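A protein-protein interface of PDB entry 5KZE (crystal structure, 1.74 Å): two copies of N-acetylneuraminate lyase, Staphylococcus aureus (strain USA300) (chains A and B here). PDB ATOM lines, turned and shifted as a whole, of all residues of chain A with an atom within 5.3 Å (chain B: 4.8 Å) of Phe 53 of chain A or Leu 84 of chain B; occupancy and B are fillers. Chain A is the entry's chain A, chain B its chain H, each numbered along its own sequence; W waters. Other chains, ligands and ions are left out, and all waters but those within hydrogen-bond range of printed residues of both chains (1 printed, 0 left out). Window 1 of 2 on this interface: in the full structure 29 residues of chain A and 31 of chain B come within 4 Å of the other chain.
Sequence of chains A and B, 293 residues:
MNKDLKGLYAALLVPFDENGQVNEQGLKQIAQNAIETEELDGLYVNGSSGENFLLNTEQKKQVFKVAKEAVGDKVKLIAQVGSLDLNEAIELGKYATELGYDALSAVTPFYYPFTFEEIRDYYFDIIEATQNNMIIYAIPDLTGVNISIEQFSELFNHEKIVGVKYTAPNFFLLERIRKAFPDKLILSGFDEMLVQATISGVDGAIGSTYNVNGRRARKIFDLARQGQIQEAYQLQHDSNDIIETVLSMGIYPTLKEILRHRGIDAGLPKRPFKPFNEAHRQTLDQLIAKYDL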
ATOM      1  N   ASN A  46     -33.093  -5.089  10.519  1.00  0.00           N
ATOM      2  CA  ASN A  46     -33.083  -4.305  11.750  1.00  0.00           C
ATOM      3  C   ASN A  46     -33.152  -5.169  13.009  1.00  0.00           C
ATOM      4  O   ASN A  46     -33.681  -4.753  14.044  1.00  0.00           O
ATOM      5  CB  ASN A  46     -34.220  -3.277  11.739  1.00  0.00           C
ATOM      6  CG  ASN A  46     -33.845  -2.000  11.007  1.00  0.00           C
ATOM      7  OD1 ASN A  46     -32.704  -1.543  11.074  1.00  0.00           O
ATOM      8  ND2 ASN A  46     -34.808  -1.410  10.311  1.00  0.00           N
ATOM      9  N   GLY A  47     -32.612  -6.375  12.921  1.00  0.00           N
ATOM     10  CA  GLY A  47     -32.398  -7.182  14.104  1.00  0.00           C
ATOM     11  C   GLY A  47     -31.194  -6.642  14.865  1.00  0.00           C
ATOM     12  O   GLY A  47     -30.615  -5.618  14.493  1.00  0.00           O
ATOM     13  N   SER A  48     -30.808  -7.335  15.928  1.00  0.00           N
ATOM     14  CA  SER A  48     -29.670  -6.908  16.733  1.00  0.00           C
ATOM     15  C   SER A  48     -28.384  -6.775  15.906  1.00  0.00           C
ATOM     16  O   SER A  48     -27.657  -5.792  16.032  1.00  0.00           O
ATOM     17  CB  SER A  48     -29.456  -7.882  17.888  1.00  0.00           C
ATOM     18  OG  SER A  48     -30.628  -7.978  18.674  1.00  0.00           O
ATOM     19  N   GLU A  51     -27.289  -3.752  14.204  1.00  0.00           N
ATOM     20  CA  GLU A  51     -27.005  -2.672  15.158  1.00  0.00           C
ATOM     21  C   GLU A  51     -28.238  -1.798  15.382  1.00  0.00           C
ATOM     22  O   GLU A  51     -28.137  -0.632  15.762  1.00  0.00           O
ATOM     23  CB  GLU A  51     -25.811  -1.842  14.681  1.00  0.00           C
ATOM     24  CG  GLU A  51     -24.519  -2.594  14.793  1.00  0.00           C
ATOM     25  CD  GLU A  51     -23.375  -1.910  14.092  1.00  0.00           C
ATOM     26  OE1 GLU A  51     -22.975  -2.400  13.012  1.00  0.00           O
ATOM     27  OE2 GLU A  51     -22.865  -0.898  14.615  1.00  0.00           O
ATOM     28  N   ASN A  52     -29.403  -2.402  15.155  1.00  0.00           N
ATOM     29  CA  ASN A  52     -30.696  -1.734  15.262  1.00  0.00           C
ATOM     30  C   ASN A  52     -30.899  -0.881  16.498  1.00  0.00           C
ATOM     31  O   ASN A  52     -31.402   0.232  16.410  1.00  0.00           O
ATOM     32  CB  ASN A  52     -31.823  -2.765  15.217  1.00  0.00           C
ATOM     33  CG  ASN A  52     -33.191  -2.134  15.397  1.00  0.00           C
ATOM     34  OD1 ASN A  52     -33.637  -1.361  14.553  1.00  0.00           O
ATOM     35  ND2 ASN A  52     -33.870  -2.469  16.493  1.00  0.00           N
ATOM     36  N   PHE A  53     -30.529  -1.398  17.659  1.00  0.00           N
ATOM     37  CA  PHE A  53     -30.919  -0.728  18.895  1.00  0.00           C
ATOM     38  C   PHE A  53     -29.999   0.454  19.211  1.00  0.00           C
ATOM     39  O   PHE A  53     -30.217   1.191  20.172  1.00  0.00           O
ATOM     40  CB  PHE A  53     -30.985  -1.767  20.018  1.00  0.00           C
ATOM     41  CG  PHE A  53     -31.973  -2.865  19.722  1.00  0.00           C
ATOM     42  CD1 PHE A  53     -33.324  -2.672  19.958  1.00  0.00           C
ATOM     43  CD2 PHE A  53     -31.561  -4.059  19.134  1.00  0.00           C
ATOM     44  CE1 PHE A  53     -34.244  -3.659  19.646  1.00  0.00           C
ATOM     45  CE2 PHE A  53     -32.479  -5.053  18.823  1.00  0.00           C
ATOM     46  CZ  PHE A  53     -33.818  -4.852  19.079  1.00  0.00           C
ATOM     47  N   LEU A  54     -29.010   0.661  18.346  1.00  0.00           N
ATOM     48  CA  LEU A  54     -28.168   1.843  18.404  1.00  0.00           C
ATOM     49  C   LEU A  54     -28.687   2.938  17.472  1.00  0.00           C
ATOM     50  O   LEU A  54     -28.098   4.009  17.386  1.00  0.00           O
ATOM     51  CB  LEU A  54     -26.718   1.501  18.032  1.00  0.00           C
ATOM     52  CG  LEU A  54     -25.990   0.350  18.741  1.00  0.00           C
ATOM     53  CD1 LEU A  54     -24.536   0.246  18.243  1.00  0.00           C
ATOM     54  CD2 LEU A  54     -26.038   0.470  20.258  1.00  0.00           C
ATOM     55  N   LEU A  55     -29.781   2.665  16.767  1.00  0.00           N
ATOM     56  CA  LEU A  55     -30.281   3.588  15.752  1.00  0.00           C
ATOM     57  C   LEU A  55     -31.415   4.482  16.250  1.00  0.00           C
ATOM     58  O   LEU A  55     -32.018   4.233  17.300  1.00  0.00           O
ATOM     59  CB  LEU A  55     -30.778   2.822  14.525  1.00  0.00           C
ATOM     60  CG  LEU A  55     -29.875   1.796  13.851  1.00  0.00           C
ATOM     61  CD1 LEU A  55     -30.590   1.224  12.638  1.00  0.00           C
ATOM     62  CD2 LEU A  55     -28.556   2.443  13.455  1.00  0.00           C
ATOM     63  N   LYS A  60     -33.794   3.548  11.088  1.00  0.00           N
ATOM     64  CA  LYS A  60     -34.395   2.226  10.982  1.00  0.00           C
ATOM     65  C   LYS A  60     -35.289   2.189   9.751  1.00  0.00           C
ATOM     66  O   LYS A  60     -35.304   1.216   9.008  1.00  0.00           O
ATOM     67  CB  LYS A  60     -35.178   1.886  12.252  1.00  0.00           C
ATOM     68  CG  LYS A  60     -34.333   1.956  13.546  1.00  0.00           C
ATOM     69  CD  LYS A  60     -35.238   1.921  14.778  1.00  0.00           C
ATOM     70  CE  LYS A  60     -34.462   1.838  16.088  1.00  0.00           C
ATOM     71  NZ  LYS A  60     -35.388   1.768  17.261  1.00  0.00           N
ATOM     72  N   GLN A  80     -37.685  -6.644  11.864  1.00  0.00           N
ATOM     73  CA  GLN A  80     -37.590  -6.516  13.318  1.00  0.00           C
ATOM     74  C   GLN A  80     -37.947  -5.091  13.705  1.00  0.00           C
ATOM     75  O   GLN A  80     -37.238  -4.159  13.355  1.00  0.00           O
ATOM     76  CB  GLN A  80     -36.200  -6.880  13.831  1.00  0.00           C
ATOM     77  CG  GLN A  80     -36.168  -7.291  15.315  1.00  0.00           C
ATOM     78  CD  GLN A  80     -36.522  -6.158  16.277  1.00  0.00           C
ATOM     79  OE1 GLN A  80     -37.262  -6.357  17.237  1.00  0.00           O
ATOM     80  NE2 GLN A  80     -35.988  -4.973  16.027  1.00  0.00           N
ATOM     81  N   GLY A  82     -39.338  -4.397  16.973  1.00  0.00           N
ATOM     82  CA  GLY A  82     -39.341  -4.320  18.418  1.00  0.00           C
ATOM     83  C   GLY A  82     -38.469  -3.190  18.921  1.00  0.00           C
ATOM     84  O   GLY A  82     -37.422  -2.899  18.352  1.00  0.00           O
ATOM     85  N   SER A  83     -38.927  -2.561  19.999  1.00  0.00           N
ATOM     86  CA  SER A  83     -38.305  -1.384  20.589  1.00  0.00           C
ATOM     87  C   SER A  83     -38.766  -1.218  22.035  1.00  0.00           C
ATOM     88  O   SER A  83     -39.834  -1.683  22.403  1.00  0.00           O
ATOM     89  CB  SER A  83     -38.656  -0.132  19.792  1.00  0.00           C
ATOM     90  OG  SER A  83     -38.265   1.038  20.500  1.00  0.00           O
ATOM     91  N   VAL A 107     -38.442  -8.037  19.384  1.00  0.00           N
ATOM     92  CA  VAL A 107     -37.708  -8.512  20.551  1.00  0.00           C
ATOM     93  C   VAL A 107     -38.561  -8.357  21.824  1.00  0.00           C
ATOM     94  O   VAL A 107     -39.339  -7.413  21.940  1.00  0.00           O
ATOM     95  CB  VAL A 107     -36.365  -7.745  20.691  1.00  0.00           C
ATOM     96  CG1 VAL A 107     -36.601  -6.333  21.182  1.00  0.00           C
ATOM     97  CG2 VAL A 107     -35.392  -8.496  21.589  1.00  0.00           C
ATOM     98  N   PHE A 110     -37.206  -5.393  27.069  1.00  0.00           N
ATOM     99  CA  PHE A 110     -36.061  -5.624  27.946  1.00  0.00           C
ATOM    100  C   PHE A 110     -35.744  -4.394  28.785  1.00  0.00           C
ATOM    101  O   PHE A 110     -36.519  -3.437  28.817  1.00  0.00           O
ATOM    102  CB  PHE A 110     -34.828  -6.040  27.132  1.00  0.00           C
ATOM    103  CG  PHE A 110     -34.455  -5.070  26.052  1.00  0.00           C
ATOM    104  CD1 PHE A 110     -35.059  -5.140  24.806  1.00  0.00           C
ATOM    105  CD2 PHE A 110     -33.488  -4.093  26.276  1.00  0.00           C
ATOM    106  CE1 PHE A 110     -34.718  -4.251  23.815  1.00  0.00           C
ATOM    107  CE2 PHE A 110     -33.141  -3.204  25.290  1.00  0.00           C
ATOM    108  CZ  PHE A 110     -33.751  -3.279  24.055  1.00  0.00           C
ATOM    109  N   TYR A 137     -39.398 -12.626  18.868  1.00  0.00           N
ATOM    110  CA  TYR A 137     -37.952 -12.543  18.819  1.00  0.00           C
ATOM    111  C   TYR A 137     -37.414 -12.803  20.231  1.00  0.00           C
ATOM    112  O   TYR A 137     -37.368 -11.906  21.060  1.00  0.00           O
ATOM    113  CB  TYR A 137     -37.556 -11.174  18.272  1.00  0.00           C
ATOM    114  CG  TYR A 137     -36.083 -10.886  18.109  1.00  0.00           C
ATOM    115  CD1 TYR A 137     -35.112 -11.843  18.379  1.00  0.00           C
ATOM    116  CD2 TYR A 137     -35.671  -9.629  17.697  1.00  0.00           C
ATOM    117  CE1 TYR A 137     -33.772 -11.556  18.237  1.00  0.00           C
ATOM    118  CE2 TYR A 137     -34.340  -9.333  17.547  1.00  0.00           C
ATOM    119  CZ  TYR A 137     -33.395 -10.296  17.822  1.00  0.00           C
ATOM    120  OH  TYR A 137     -32.069  -9.980  17.662  1.00  0.00           O
ATOM    121  N   ARG A 271     -20.792   3.824  16.725  1.00  0.00           N
ATOM    122  CA  ARG A 271     -20.264   3.996  18.072  1.00  0.00           C
ATOM    123  C   ARG A 271     -21.408   3.791  19.051  1.00  0.00           C
ATOM    124  O   ARG A 271     -22.532   4.160  18.758  1.00  0.00           O
ATOM    125  CB  ARG A 271     -19.618   5.375  18.243  1.00  0.00           C
ATOM    126  CG  ARG A 271     -18.237   5.500  17.609  1.00  0.00           C
ATOM    127  CD  ARG A 271     -17.607   6.863  17.882  1.00  0.00           C
ATOM    128  NE  ARG A 271     -18.429   7.965  17.396  1.00  0.00           N
ATOM    129  CZ  ARG A 271     -18.052   8.834  16.461  1.00  0.00           C
ATOM    130  NH1 ARG A 271     -16.849   8.731  15.906  1.00  0.00           N
ATOM    131  NH2 ARG A 271     -18.873   9.811  16.086  1.00  0.00           N
ATOM    132  N   PRO A 272     -21.124   3.221  20.233  1.00  0.00           N
ATOM    133  CA  PRO A 272     -19.806   2.995  20.834  1.00  0.00           C
ATOM    134  C   PRO A 272     -19.072   1.717  20.412  1.00  0.00           C
ATOM    135  O   PRO A 272     -18.026   1.445  20.985  1.00  0.00           O
ATOM    136  CB  PRO A 272     -20.121   2.942  22.340  1.00  0.00           C
ATOM    137  CG  PRO A 272     -21.619   2.798  22.455  1.00  0.00           C
ATOM    138  CD  PRO A 272     -22.190   2.664  21.074  1.00  0.00           C
ATOM    139  N   GLY B  82     -27.953   9.114  29.098  1.00  0.00           N
ATOM    140  CA  GLY B  82     -27.430   7.883  28.546  1.00  0.00           C
ATOM    141  C   GLY B  82     -28.444   7.220  27.634  1.00  0.00           C
ATOM    142  O   GLY B  82     -29.644   7.368  27.831  1.00  0.00           O
ATOM    143  N   SER B  83     -27.957   6.483  26.647  1.00  0.00           N
ATOM    144  CA  SER B  83     -28.809   5.892  25.615  1.00  0.00           C
ATOM    145  C   SER B  83     -27.986   4.918  24.773  1.00  0.00           C
ATOM    146  O   SER B  83     -26.781   5.091  24.637  1.00  0.00           O
ATOM    147  CB  SER B  83     -29.418   6.987  24.734  1.00  0.00           C
ATOM    148  OG  SER B  83     -30.174   6.447  23.663  1.00  0.00           O
ATOM    149  N   LEU B  84     -28.634   3.892  24.221  1.00  0.00           N
ATOM    150  CA  LEU B  84     -27.963   2.957  23.321  1.00  0.00           C
ATOM    151  C   LEU B  84     -27.542   3.655  22.031  1.00  0.00           C
ATOM    152  O   LEU B  84     -26.651   3.186  21.326  1.00  0.00           O
ATOM    153  CB  LEU B  84     -28.866   1.763  23.005  1.00  0.00           C
ATOM    154  CG  LEU B  84     -29.136   0.804  24.168  1.00  0.00           C
ATOM    155  CD1 LEU B  84     -29.673  -0.530  23.658  1.00  0.00           C
ATOM    156  CD2 LEU B  84     -27.890   0.602  25.012  1.00  0.00           C
ATOM    157  N   ASP B  85     -28.191   4.776  21.738  1.00  0.00           N
ATOM    158  CA  ASP B  85     -27.826   5.635  20.616  1.00  0.00           C
ATOM    159  C   ASP B  85     -26.950   6.768  21.147  1.00  0.00           C
ATOM    160  O   ASP B  85     -27.463   7.739  21.710  1.00  0.00           O
ATOM    161  CB  ASP B  85     -29.085   6.185  19.925  1.00  0.00           C
ATOM    162  CG  ASP B  85     -28.774   7.113  18.737  1.00  0.00           C
ATOM    163  OD1 ASP B  85     -27.601   7.464  18.505  1.00  0.00           O
ATOM    164  OD2 ASP B  85     -29.721   7.511  18.029  1.00  0.00           O
ATOM    165  N   LEU B  86     -25.636   6.641  20.967  1.00  0.00           N
ATOM    166  CA  LEU B  86     -24.693   7.654  21.442  1.00  0.00           C
ATOM    167  C   LEU B  86     -24.956   9.038  20.854  1.00  0.00           C
ATOM    168  O   LEU B  86     -24.805  10.045  21.549  1.00  0.00           O
ATOM    169  CB  LEU B  86     -23.253   7.237  21.138  1.00  0.00           C
ATOM    170  CG  LEU B  86     -22.146   8.229  21.507  1.00  0.00           C
ATOM    171  CD1 LEU B  86     -22.115   8.509  22.994  1.00  0.00           C
ATOM    172  CD2 LEU B  86     -20.807   7.704  21.056  1.00  0.00           C
ATOM    173  N   PRO B 109     -23.617   1.698  28.678  1.00  0.00           N
ATOM    174  CA  PRO B 109     -24.185   1.040  27.497  1.00  0.00           C
ATOM    175  C   PRO B 109     -24.549  -0.430  27.772  1.00  0.00           C
ATOM    176  O   PRO B 109     -23.781  -1.153  28.404  1.00  0.00           O
ATOM    177  CB  PRO B 109     -23.061   1.163  26.467  1.00  0.00           C
ATOM    178  CG  PRO B 109     -22.387   2.422  26.839  1.00  0.00           C
ATOM    179  CD  PRO B 109     -22.400   2.453  28.346  1.00  0.00           C
ATOM    180  N   PHE B 110     -25.729  -0.847  27.322  1.00  0.00           N
ATOM    181  CA  PHE B 110     -26.254  -2.170  27.644  1.00  0.00           C
ATOM    182  C   PHE B 110     -26.842  -2.867  26.424  1.00  0.00           C
ATOM    183  O   PHE B 110     -26.638  -2.434  25.288  1.00  0.00           O
ATOM    184  CB  PHE B 110     -27.320  -2.076  28.750  1.00  0.00           C
ATOM    185  CG  PHE B 110     -28.473  -1.183  28.407  1.00  0.00           C
ATOM    186  CD1 PHE B 110     -28.364   0.196  28.543  1.00  0.00           C
ATOM    187  CD2 PHE B 110     -29.675  -1.718  27.959  1.00  0.00           C
ATOM    188  CE1 PHE B 110     -29.423   1.028  28.228  1.00  0.00           C
ATOM    189  CE2 PHE B 110     -30.734  -0.896  27.644  1.00  0.00           C
ATOM    190  CZ  PHE B 110     -30.609   0.489  27.776  1.00  0.00           C
ATOM    191  N   TYR B 111     -27.589  -3.939  26.686  1.00  0.00           N
ATOM    192  CA  TYR B 111     -28.149  -4.806  25.654  1.00  0.00           C
ATOM    193  C   TYR B 111     -27.047  -5.581  24.939  1.00  0.00           C
ATOM    194  O   TYR B 111     -26.963  -6.804  25.060  1.00  0.00           O
ATOM    195  CB  TYR B 111     -28.982  -4.020  24.633  1.00  0.00           C
ATOM    196  CG  TYR B 111     -29.699  -4.956  23.690  1.00  0.00           C
ATOM    197  CD1 TYR B 111     -30.803  -5.703  24.117  1.00  0.00           C
ATOM    198  CD2 TYR B 111     -29.243  -5.143  22.392  1.00  0.00           C
ATOM    199  CE1 TYR B 111     -31.442  -6.587  23.261  1.00  0.00           C
ATOM    200  CE2 TYR B 111     -29.878  -6.021  21.534  1.00  0.00           C
ATOM    201  CZ  TYR B 111     -30.968  -6.739  21.971  1.00  0.00           C
ATOM    202  OH  TYR B 111     -31.575  -7.607  21.097  1.00  0.00           O
ATOM    203  N   TYR B 112     -26.201  -4.867  24.198  1.00  0.00           N
ATOM    204  CA  TYR B 112     -25.063  -5.463  23.512  1.00  0.00           C
ATOM    205  C   TYR B 112     -23.918  -5.744  24.485  1.00  0.00           C
ATOM    206  O   TYR B 112     -23.775  -5.038  25.481  1.00  0.00           O
ATOM    207  CB  TYR B 112     -24.567  -4.541  22.402  1.00  0.00           C
ATOM    208  CG  TYR B 112     -25.511  -4.353  21.234  1.00  0.00           C
ATOM    209  CD1 TYR B 112     -25.710  -5.369  20.308  1.00  0.00           C
ATOM    210  CD2 TYR B 112     -26.171  -3.143  21.033  1.00  0.00           C
ATOM    211  CE1 TYR B 112     -26.560  -5.194  19.216  1.00  0.00           C
ATOM    212  CE2 TYR B 112     -27.019  -2.959  19.941  1.00  0.00           C
ATOM    213  CZ  TYR B 112     -27.206  -3.988  19.040  1.00  0.00           C
ATOM    214  OH  TYR B 112     -28.044  -3.803  17.968  1.00  0.00           O
HETATM  215  O   HOH W   1     -24.996   4.344  19.321  1.00  0.00           O
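Water W1 lies within hydrogen-bond range of O of Arg 271 of chain A (2.5 Å), O of Leu 84 of chain B (2.8 Å) and N of Leu 86 of chain B (2.9 Å).
Positions printed for both chains: 82, 83 and 110.
Of the 14 pairs that touch across the chains among the printed residues, none has its exchanged pair printed and touching as well.
Glu 51 of chain A touches Tyr 112 of chain B (CA to OH, 3.2 Å).
Leu 84 of chain B touches Phe 53 of chain A (CB to O, 3.2 Å).
Phe 53 of chain A touches Tyr 111 of chain B.
Leu 84 of chain B touches Leu 54 of chain A (O to CD2, 3.0 Å).
Asp 85 of chain B touches Leu 54 of chain A.
CE2 of Tyr 112 of chain B touches CD2 of Leu 54 of chain A (3.6 Å).
Leu 55 of chain A touches Asp 85 of chain B (C to OD2, 3.9 Å).
CG2 of Val 107 of chain A touches OH of Tyr 111 of chain B, at 3.9 Å.
Tyr 111 of chain B touches Phe 110 of chain A (CD1 to CE2, 3.6 Å).
Arg 271 of chain A touches Leu 86 of chain B (CB to CD2, 3.8 Å).
The side-chain hydroxyl (OG) of Ser 48 of chain A is in hydrogen-bond range of the side-chain hydroxyl (OH) of Tyr 111 of chain B (2.6 Å).
O of Ser 48 of chain A lies within hydrogen-bond range of OH of Tyr 112 of chain B (2.8 Å).
The side-chain hydroxyl (OH) of Tyr 112 of chain B sits at hydrogen-bond distance from the backbone NH (N) of Phe 53 of chain A (3.5 Å).
N of Asn 52 of chain A sits at hydrogen-bond distance from OH of Tyr 112 of chain B (3.4 Å).
Printed residues of chain A that touch a printed residue of chain B: Ser 48, Glu 51, Asn 52, Phe 53, Leu 54, Leu 55, Val 107, Phe 110 and Arg 271.
Hydrophobic or aromatic side chains of chain A that line the printed part of chain B: Phe 53, Leu 54, Val 107 and Phe 110.
Among the printed residues, 14 pairs touch across the chains.
Among the printed residues, no Asp or Glu carboxylate lies within 4 Å of a Lys or Arg side-chain nitrogen of the other chain.
OG of Ser 48 of chain A lies within hydrogen-bond range of OH of Tyr 137 of chain A, 2.7 Å away.
The backbone NH of Val 107 of chain A sits at hydrogen-bond distance from the side-chain amide oxygen of Gln 80 of chain A (3.0 Å).
The side-chain hydroxyl (OG) of Ser 83 of chain B sits close to the backbone NH (N) of Asp 85 of chain B, 3.2 Å away.
The side-chain amide nitrogen of Asn 52 of chain A sits close to the side-chain amide nitrogen of Gln 80 of chain A, at 3.3 Å.
The backbone carbonyl oxygen (O) of Asn 46 of chain A lies close to the side-chain amide nitrogen (ND2) of Asn 52 of chain A.
Phe 53 of chain A touches three residues of chain B.
Of the printed residues of chain B, Val 107 of chain A touches Tyr 111.
Of the printed residues of chain B, Phe 110 of chain A touches Tyr 111.
Of the printed residues of chain B, Arg 271 of chain A touches Leu 86.
Leu 84 of chain B touches just these residues of chain A: Phe 53 and Leu 54.
Printed residues of chain A within 4 Å of Asp 85 of chain B: Leu 54 (3.5 Å) and Leu 55 (3.9 Å).
Printed residues of chain A within 4 Å of Leu 86 of chain B: Arg 271.
Pro 109 of chain B touches none of the printed residues of chain A.
The nearest printed residue of chain B that does not touch Leu 54 of chain A is Leu 86 of chain B (5.1 Å).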
